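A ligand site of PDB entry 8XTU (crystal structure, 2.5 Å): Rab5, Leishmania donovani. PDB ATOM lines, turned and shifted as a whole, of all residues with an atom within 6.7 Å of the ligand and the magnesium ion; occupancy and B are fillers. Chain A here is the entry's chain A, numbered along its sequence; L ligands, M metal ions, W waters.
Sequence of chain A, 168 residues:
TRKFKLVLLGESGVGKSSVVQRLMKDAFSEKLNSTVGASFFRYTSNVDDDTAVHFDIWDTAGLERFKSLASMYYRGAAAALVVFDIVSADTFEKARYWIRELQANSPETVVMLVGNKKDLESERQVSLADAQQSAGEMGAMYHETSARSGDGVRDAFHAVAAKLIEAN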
ATOM      1  N   GLY A  10      28.395  12.729 -34.284  1.00  0.00           N
ATOM      2  CA  GLY A  10      28.756  12.417 -32.909  1.00  0.00           C
ATOM      3  C   GLY A  10      29.691  11.206 -32.891  1.00  0.00           C
ATOM      4  O   GLY A  10      29.858  10.565 -33.916  1.00  0.00           O
ATOM      5  N   GLU A  11      30.281  10.914 -31.718  1.00  0.00           N
ATOM      6  CA  GLU A  11      31.238   9.829 -31.568  1.00  0.00           C
ATOM      7  C   GLU A  11      30.531   8.496 -31.762  1.00  0.00           C
ATOM      8  O   GLU A  11      29.304   8.436 -31.771  1.00  0.00           O
ATOM      9  CB  GLU A  11      31.900   9.843 -30.186  1.00  0.00           C
ATOM     10  CG  GLU A  11      32.992  10.882 -30.039  1.00  0.00           C
ATOM     11  CD  GLU A  11      34.087  10.890 -31.087  1.00  0.00           C
ATOM     12  OE1 GLU A  11      34.285  11.951 -31.734  1.00  0.00           O
ATOM     13  OE2 GLU A  11      34.712   9.807 -31.311  1.00  0.00           O
ATOM     14  N   SER A  12      31.322   7.443 -31.910  1.00  0.00           N
ATOM     15  CA  SER A  12      30.752   6.115 -32.065  1.00  0.00           C
ATOM     16  C   SER A  12      30.189   5.643 -30.723  1.00  0.00           C
ATOM     17  O   SER A  12      30.765   5.926 -29.679  1.00  0.00           O
ATOM     18  CB  SER A  12      31.798   5.182 -32.581  1.00  0.00           C
ATOM     19  OG  SER A  12      33.062   5.582 -32.087  1.00  0.00           O
ATOM     20  N   GLY A  13      29.039   4.975 -30.760  1.00  0.00           N
ATOM     21  CA  GLY A  13      28.456   4.359 -29.582  1.00  0.00           C
ATOM     22  C   GLY A  13      27.626   5.314 -28.732  1.00  0.00           C
ATOM     23  O   GLY A  13      27.073   4.909 -27.700  1.00  0.00           O
ATOM     24  N   VAL A  14      27.521   6.578 -29.160  1.00  0.00           N
ATOM     25  CA  VAL A  14      26.727   7.567 -28.456  1.00  0.00           C
ATOM     26  C   VAL A  14      25.221   7.282 -28.617  1.00  0.00           C
ATOM     27  O   VAL A  14      24.431   7.669 -27.742  1.00  0.00           O
ATOM     28  CB  VAL A  14      27.087   9.009 -28.866  1.00  0.00           C
ATOM     29  CG1 VAL A  14      28.568   9.317 -28.657  1.00  0.00           C
ATOM     30  CG2 VAL A  14      26.633   9.324 -30.292  1.00  0.00           C
ATOM     31  N   GLY A  15      24.829   6.618 -29.721  1.00  0.00           N
ATOM     32  CA  GLY A  15      23.478   6.098 -29.918  1.00  0.00           C
ATOM     33  C   GLY A  15      22.767   6.624 -31.173  1.00  0.00           C
ATOM     34  O   GLY A  15      21.554   6.467 -31.308  1.00  0.00           O
ATOM     35  N   LYS A  16      23.545   7.210 -32.098  1.00  0.00           N
ATOM     36  CA  LYS A  16      23.020   7.806 -33.309  1.00  0.00           C
ATOM     37  C   LYS A  16      22.083   6.802 -33.995  1.00  0.00           C
ATOM     38  O   LYS A  16      20.905   7.091 -34.193  1.00  0.00           O
ATOM     39  CB  LYS A  16      24.121   8.165 -34.312  1.00  0.00           C
ATOM     40  CG  LYS A  16      25.023   9.342 -33.941  1.00  0.00           C
ATOM     41  CD  LYS A  16      26.164   9.574 -34.893  1.00  0.00           C
ATOM     42  CE  LYS A  16      27.021   8.358 -35.201  1.00  0.00           C
ATOM     43  NZ  LYS A  16      27.913   7.963 -34.065  1.00  0.00           N
ATOM     44  N   SER A  17      22.653   5.646 -34.352  1.00  0.00           N
ATOM     45  CA  SER A  17      21.889   4.635 -35.085  1.00  0.00           C
ATOM     46  C   SER A  17      20.629   4.241 -34.301  1.00  0.00           C
ATOM     47  O   SER A  17      19.583   4.058 -34.928  1.00  0.00           O
ATOM     48  CB  SER A  17      22.747   3.438 -35.382  1.00  0.00           C
ATOM     49  OG  SER A  17      24.063   3.851 -35.747  1.00  0.00           O
ATOM     50  N   SER A  18      20.747   4.118 -32.976  1.00  0.00           N
ATOM     51  CA  SER A  18      19.598   3.691 -32.172  1.00  0.00           C
ATOM     52  C   SER A  18      18.545   4.802 -32.111  1.00  0.00           C
ATOM     53  O   SER A  18      17.347   4.498 -32.073  1.00  0.00           O
ATOM     54  CB  SER A  18      20.036   3.263 -30.809  1.00  0.00           C
ATOM     55  OG  SER A  18      21.164   2.403 -30.904  1.00  0.00           O
ATOM     56  N   VAL A  19      18.980   6.067 -32.108  1.00  0.00           N
ATOM     57  CA  VAL A  19      18.036   7.161 -32.007  1.00  0.00           C
ATOM     58  C   VAL A  19      17.070   7.096 -33.176  1.00  0.00           C
ATOM     59  O   VAL A  19      15.873   7.346 -33.019  1.00  0.00           O
ATOM     60  CB  VAL A  19      18.721   8.537 -31.921  1.00  0.00           C
ATOM     61  CG1 VAL A  19      17.702   9.675 -32.048  1.00  0.00           C
ATOM     62  CG2 VAL A  19      19.497   8.678 -30.630  1.00  0.00           C
ATOM     63  N   GLN A  21      16.546   4.491 -35.471  1.00  0.00           N
ATOM     64  CA  GLN A  21      15.763   3.270 -35.379  1.00  0.00           C
ATOM     65  C   GLN A  21      14.574   3.511 -34.454  1.00  0.00           C
ATOM     66  O   GLN A  21      13.432   3.321 -34.862  1.00  0.00           O
ATOM     67  CB  GLN A  21      16.630   2.074 -34.976  1.00  0.00           C
ATOM     68  CG  GLN A  21      17.592   1.659 -36.089  1.00  0.00           C
ATOM     69  CD  GLN A  21      18.823   0.914 -35.601  1.00  0.00           C
ATOM     70  OE1 GLN A  21      18.849   0.338 -34.518  1.00  0.00           O
ATOM     71  N   ASP A  59      22.399   8.480 -41.563  1.00  0.00           N
ATOM     72  CA  ASP A  59      23.152   7.929 -40.457  1.00  0.00           C
ATOM     73  C   ASP A  59      24.452   7.339 -41.003  1.00  0.00           C
ATOM     74  O   ASP A  59      24.458   6.730 -42.059  1.00  0.00           O
ATOM     75  CB  ASP A  59      22.304   6.910 -39.693  1.00  0.00           C
ATOM     76  CG  ASP A  59      23.056   6.188 -38.589  1.00  0.00           C
ATOM     77  OD1 ASP A  59      23.982   6.814 -38.000  1.00  0.00           O
ATOM     78  OD2 ASP A  59      22.692   5.017 -38.299  1.00  0.00           O
ATOM     79  N   THR A  60      25.543   7.513 -40.240  1.00  0.00           N
ATOM     80  CA  THR A  60      26.906   7.401 -40.749  1.00  0.00           C
ATOM     81  C   THR A  60      27.632   6.223 -40.122  1.00  0.00           C
ATOM     82  O   THR A  60      27.182   5.702 -39.103  1.00  0.00           O
ATOM     83  CB  THR A  60      27.703   8.679 -40.469  1.00  0.00           C
ATOM     84  OG1 THR A  60      28.889   8.720 -41.256  1.00  0.00           O
ATOM     85  N   ALA A  61      28.776   5.869 -40.740  1.00  0.00           N
ATOM     86  CA  ALA A  61      29.652   4.749 -40.367  1.00  0.00           C
ATOM     87  C   ALA A  61      31.067   5.189 -39.978  1.00  0.00           C
ATOM     88  O   ALA A  61      31.670   4.489 -39.157  1.00  0.00           O
ATOM     89  CB  ALA A  61      29.681   3.744 -41.490  1.00  0.00           C
ATOM     90  N   VAL A  83      24.913  14.142 -31.486  1.00  0.00           N
ATOM     91  CA  VAL A  83      24.640  13.356 -30.303  1.00  0.00           C
ATOM     92  C   VAL A  83      25.943  13.142 -29.543  1.00  0.00           C
ATOM     93  O   VAL A  83      27.007  12.920 -30.131  1.00  0.00           O
ATOM     94  CB  VAL A  83      24.042  11.996 -30.703  1.00  0.00           C
ATOM     95  CG1 VAL A  83      23.466  11.275 -29.491  1.00  0.00           C
ATOM     96  CG2 VAL A  83      22.983  12.170 -31.783  1.00  0.00           C
ATOM     97  N   ASP A  85      26.940  11.114 -25.555  1.00  0.00           N
ATOM     98  CA  ASP A  85      26.488  10.222 -24.505  1.00  0.00           C
ATOM     99  C   ASP A  85      26.561  10.984 -23.181  1.00  0.00           C
ATOM    100  O   ASP A  85      27.610  11.515 -22.813  1.00  0.00           O
ATOM    101  CB  ASP A  85      27.384   8.989 -24.516  1.00  0.00           C
ATOM    102  CG  ASP A  85      26.984   7.965 -23.472  1.00  0.00           C
ATOM    103  OD1 ASP A  85      26.022   8.240 -22.728  1.00  0.00           O
ATOM    104  OD2 ASP A  85      27.630   6.902 -23.448  1.00  0.00           O
ATOM    105  N   ASN A 116      21.922  12.150 -25.320  1.00  0.00           N
ATOM    106  CA  ASN A 116      21.331  10.831 -25.432  1.00  0.00           C
ATOM    107  C   ASN A 116      21.795   9.943 -24.274  1.00  0.00           C
ATOM    108  O   ASN A 116      22.820  10.268 -23.646  1.00  0.00           O
ATOM    109  CB  ASN A 116      21.637  10.224 -26.799  1.00  0.00           C
ATOM    110  CG  ASN A 116      20.922   8.914 -26.998  1.00  0.00           C
ATOM    111  OD1 ASN A 116      19.701   8.875 -26.874  1.00  0.00           O
ATOM    112  ND2 ASN A 116      21.679   7.841 -27.219  1.00  0.00           N
ATOM    113  N   LYS A 117      21.075   8.821 -24.069  1.00  0.00           N
ATOM    114  CA  LYS A 117      21.200   7.910 -22.940  1.00  0.00           C
ATOM    115  C   LYS A 117      20.645   8.508 -21.640  1.00  0.00           C
ATOM    116  O   LYS A 117      21.099   8.156 -20.568  1.00  0.00           O
ATOM    117  CB  LYS A 117      22.652   7.460 -22.664  1.00  0.00           C
ATOM    118  CG  LYS A 117      23.137   6.233 -23.406  1.00  0.00           C
ATOM    119  CD  LYS A 117      23.806   6.513 -24.725  1.00  0.00           C
ATOM    120  CE  LYS A 117      24.497   5.294 -25.324  1.00  0.00           C
ATOM    121  NZ  LYS A 117      25.784   4.930 -24.670  1.00  0.00           N
ATOM    122  N   LYS A 118      19.656   9.402 -21.743  1.00  0.00           N
ATOM    123  CA  LYS A 118      19.090  10.087 -20.597  1.00  0.00           C
ATOM    124  C   LYS A 118      18.449   9.086 -19.612  1.00  0.00           C
ATOM    125  O   LYS A 118      18.162   9.424 -18.467  1.00  0.00           O
ATOM    126  CB  LYS A 118      18.185  11.243 -21.061  1.00  0.00           C
ATOM    127  CG  LYS A 118      16.749  10.925 -21.459  1.00  0.00           C
ATOM    128  CD  LYS A 118      15.950  12.091 -22.063  1.00  0.00           C
ATOM    129  CE  LYS A 118      15.433  13.146 -21.096  1.00  0.00           C
ATOM    130  N   ASP A 119      18.257   7.833 -20.055  1.00  0.00           N
ATOM    131  CA  ASP A 119      17.720   6.789 -19.214  1.00  0.00           C
ATOM    132  C   ASP A 119      18.699   6.461 -18.090  1.00  0.00           C
ATOM    133  O   ASP A 119      18.290   5.930 -17.057  1.00  0.00           O
ATOM    134  CB  ASP A 119      17.372   5.539 -20.037  1.00  0.00           C
ATOM    135  CG  ASP A 119      18.533   5.082 -20.902  1.00  0.00           C
ATOM    136  OD1 ASP A 119      18.859   5.809 -21.874  1.00  0.00           O
ATOM    137  OD2 ASP A 119      19.124   4.023 -20.601  1.00  0.00           O
ATOM    138  N   LEU A 120      19.993   6.777 -18.296  1.00  0.00           N
ATOM    139  CA  LEU A 120      21.019   6.483 -17.290  1.00  0.00           C
ATOM    140  C   LEU A 120      21.223   7.698 -16.392  1.00  0.00           C
ATOM    141  O   LEU A 120      22.291   8.302 -16.387  1.00  0.00           O
ATOM    142  CB  LEU A 120      22.314   6.055 -17.998  1.00  0.00           C
ATOM    143  CG  LEU A 120      22.135   4.989 -19.086  1.00  0.00           C
ATOM    144  CD1 LEU A 120      23.475   4.649 -19.706  1.00  0.00           C
ATOM    145  CD2 LEU A 120      21.500   3.733 -18.514  1.00  0.00           C
ATOM    146  N   THR A 145      17.632  12.781 -25.011  1.00  0.00           N
ATOM    147  CA  THR A 145      16.787  11.686 -25.497  1.00  0.00           C
ATOM    148  C   THR A 145      17.224  10.349 -24.898  1.00  0.00           C
ATOM    149  O   THR A 145      18.368  10.258 -24.448  1.00  0.00           O
ATOM    150  CB  THR A 145      16.896  11.505 -27.016  1.00  0.00           C
ATOM    151  OG1 THR A 145      18.253  11.202 -27.334  1.00  0.00           O
ATOM    152  CG2 THR A 145      16.426  12.710 -27.803  1.00  0.00           C
ATOM    153  N   SER A 146      16.296   9.383 -24.840  1.00  0.00           N
ATOM    154  CA  SER A 146      16.630   8.001 -24.477  1.00  0.00           C
ATOM    155  C   SER A 146      16.122   7.174 -25.641  1.00  0.00           C
ATOM    156  O   SER A 146      14.924   7.195 -25.886  1.00  0.00           O
ATOM    157  CB  SER A 146      15.980   7.555 -23.221  1.00  0.00           C
ATOM    158  OG  SER A 146      16.082   6.154 -23.091  1.00  0.00           O
ATOM    159  N   ALA A 147      17.016   6.536 -26.379  1.00  0.00           N
ATOM    160  CA  ALA A 147      16.611   5.826 -27.596  1.00  0.00           C
ATOM    161  C   ALA A 147      15.970   4.470 -27.256  1.00  0.00           C
ATOM    162  O   ALA A 147      15.401   3.856 -28.162  1.00  0.00           O
ATOM    163  CB  ALA A 147      17.810   5.671 -28.474  1.00  0.00           C
ATOM    164  N   ARG A 148      16.089   4.019 -26.009  1.00  0.00           N
ATOM    165  CA  ARG A 148      15.498   2.740 -25.573  1.00  0.00           C
ATOM    166  C   ARG A 148      14.082   2.998 -25.076  1.00  0.00           C
ATOM    167  O   ARG A 148      13.165   2.287 -25.475  1.00  0.00           O
ATOM    168  CB  ARG A 148      16.378   2.103 -24.502  1.00  0.00           C
ATOM    169  CG  ARG A 148      17.674   1.509 -25.039  1.00  0.00           C
ATOM    170  CD  ARG A 148      17.807   0.020 -24.698  1.00  0.00           C
ATOM    171  NE  ARG A 148      19.132  -0.565 -24.870  1.00  0.00           N
ATOM    172  CZ  ARG A 148      20.247  -0.076 -24.325  1.00  0.00           C
ATOM    173  N   SER A 149      13.928   4.040 -24.255  1.00  0.00           N
ATOM    174  CA  SER A 149      12.591   4.435 -23.798  1.00  0.00           C
ATOM    175  C   SER A 149      11.883   5.235 -24.892  1.00  0.00           C
ATOM    176  O   SER A 149      10.670   5.404 -24.818  1.00  0.00           O
ATOM    177  CB  SER A 149      12.706   5.245 -22.552  1.00  0.00           C
ATOM    178  OG  SER A 149      11.694   6.226 -22.489  1.00  0.00           O
ATOM    179  N   GLY A 150      12.653   5.773 -25.857  1.00  0.00           N
ATOM    180  CA  GLY A 150      12.071   6.632 -26.878  1.00  0.00           C
ATOM    181  C   GLY A 150      11.671   7.961 -26.264  1.00  0.00           C
ATOM    182  O   GLY A 150      10.999   8.753 -26.925  1.00  0.00           O
HETATM  183  P1  LIG L   1      26.170   4.854 -32.657  1.00  0.00           P
HETATM  184  O1  LIG L   1      25.236   4.797 -33.844  1.00  0.00           O
HETATM  185  O2  LIG L   1      26.360   6.246 -32.134  1.00  0.00           O
HETATM  186  O3  LIG L   1      27.479   4.142 -32.875  1.00  0.00           O
HETATM  187  O4  LIG L   1      25.441   4.039 -31.487  1.00  0.00           O
HETATM  188  P2  LIG L   1      24.454   2.761 -31.550  1.00  0.00           P
HETATM  189  O5  LIG L   1      25.149   1.638 -32.256  1.00  0.00           O
HETATM  190  O6  LIG L   1      23.119   3.227 -32.055  1.00  0.00           O
HETATM  191  O7  LIG L   1      24.317   2.383 -29.997  1.00  0.00           O
HETATM  192  C1  LIG L   1      25.539   2.267 -29.200  1.00  0.00           C
HETATM  193  C2  LIG L   1      25.279   1.527 -27.905  1.00  0.00           C
HETATM  194  O8  LIG L   1      24.560   2.403 -26.996  1.00  0.00           O
HETATM  195  C3  LIG L   1      24.440   0.243 -28.013  1.00  0.00           C
HETATM  196  O9  LIG L   1      24.917  -0.736 -27.098  1.00  0.00           O
HETATM  197  C4  LIG L   1      23.033   0.766 -27.693  1.00  0.00           C
HETATM  198  O10 LIG L   1      22.106  -0.144 -27.126  1.00  0.00           O
HETATM  199  C5  LIG L   1      23.340   1.816 -26.639  1.00  0.00           C
HETATM  200  N1  LIG L   1      22.314   2.845 -26.571  1.00  0.00           N
HETATM  201  C6  LIG L   1      21.818   3.600 -27.605  1.00  0.00           C
HETATM  202  N2  LIG L   1      20.887   4.437 -27.230  1.00  0.00           N
HETATM  203  C7  LIG L   1      20.767   4.231 -25.872  1.00  0.00           C
HETATM  204  C8  LIG L   1      19.929   4.851 -24.903  1.00  0.00           C
HETATM  205  O11 LIG L   1      19.080   5.742 -25.065  1.00  0.00           O
HETATM  206  N3  LIG L   1      20.137   4.320 -23.632  1.00  0.00           N
HETATM  207  C9  LIG L   1      21.039   3.332 -23.302  1.00  0.00           C
HETATM  208  N4  LIG L   1      21.121   2.953 -22.025  1.00  0.00           N
HETATM  209  N5  LIG L   1      21.850   2.767 -24.208  1.00  0.00           N
HETATM  210  C10 LIG L   1      21.629   3.232 -25.457  1.00  0.00           C
HETATM  211 MG    MG M   1      26.024   4.018 -35.515  1.00  0.00          MG
HETATM  212  O   HOH W   1      27.723   3.840 -36.172  1.00  0.00           O
HETATM  213  O   HOH W   2      25.837   2.043 -34.873  1.00  0.00           O
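An oxygen (O6) of the ligand lies close to the backbone NH of Ser 17 (3.4 Å). The backbone NH of Ser 18 is in hydrogen-bond range of an oxygen (O6) of the ligand, at 2.7 Å. An oxygen (O6) of the ligand lies within hydrogen-bond range of the side-chain hydroxyl (OG) of Ser 18 (2.4 Å). An oxygen (O11) of the ligand sits at hydrogen-bond distance from the backbone NH of Ala 147 (2.6 Å). The side-chain carboxylate (OD1) of Asp 119 is in hydrogen-bond range of a nitrogen (N3) of the ligand, 2.6 Å away. N of Gly 13 lies within hydrogen-bond range of O3 of the ligand (2.8 Å). An oxygen (O2) of the ligand lies within hydrogen-bond range of the backbone NH (N) of Gly 15 (2.9 Å). N of Lys 16 is in hydrogen-bond range of O2 of the ligand (3.0 Å). The side-chain amino group (NZ) of Lys 16 is in salt-bridge range of an oxygen (O2) of the ligand, at 3.0 Å. An oxygen (O2) of the ligand is in hydrogen-bond range of the backbone NH of Val 14 (3.2 Å). The side-chain amide nitrogen (ND2) of Asn 116 lies within hydrogen-bond range of a nitrogen (N2) of the ligand.
OG of Ser 17 lies close to OD2 of Asp 59 (3.1 Å). The side-chain hydroxyl (OG) of Ser 146 sits at hydrogen-bond distance from the side-chain carboxylate (OD1) of Asp 119. NZ of Lys 16 lies within hydrogen-bond range of O of Glu 11, at 2.7 Å. The backbone carbonyl oxygen (O) of Val 14 is in hydrogen-bond range of the side-chain amide nitrogen (ND2) of Asn 116, at 2.8 Å. OG of Ser 146 is in hydrogen-bond range of N of Ser 149 (3.2 Å). The backbone carbonyl oxygen of Thr 145 lies within hydrogen-bond range of the backbone NH of Lys 117, 3.1 Å away. NZ of Lys 117 lies within salt-bridge range of OD2 of Asp 85 (3.0 Å). The side-chain hydroxyl of Thr 145 lies within hydrogen-bond range of the side-chain amide oxygen of Asn 116 (2.8 Å).
O of Glu 11 touches O2 of the ligand, 3.7 Å away. Ser 12 touches the ligand. Lys 117 touches the ligand. CD2 of Leu 120 touches N4 of the ligand, at 3.6 Å. Ser 146 touches the ligand (C to O11, 3.3 Å). Arg 148 touches the ligand (CZ to N5, 3.3 Å). Within 4 Å of the ligand: Glu 11, Ser 12, Gly 13, Val 14, Gly 15, Lys 16, Ser 17, Ser 18, Asn 116, Lys 117, Asp 119, Leu 120, Ser 146, Ala 147 and Arg 148.
Of the 27 residues printed, 1 comes within 4 Å of the magnesium ion.
The magnesium ion is bound by water W1 (1.8 Å), OG of Ser 17 (2.0 Å), O1 of the ligand (2.0 Å) and water W2 (2.1 Å). The magnesium ion has four donor atoms within binding distance.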
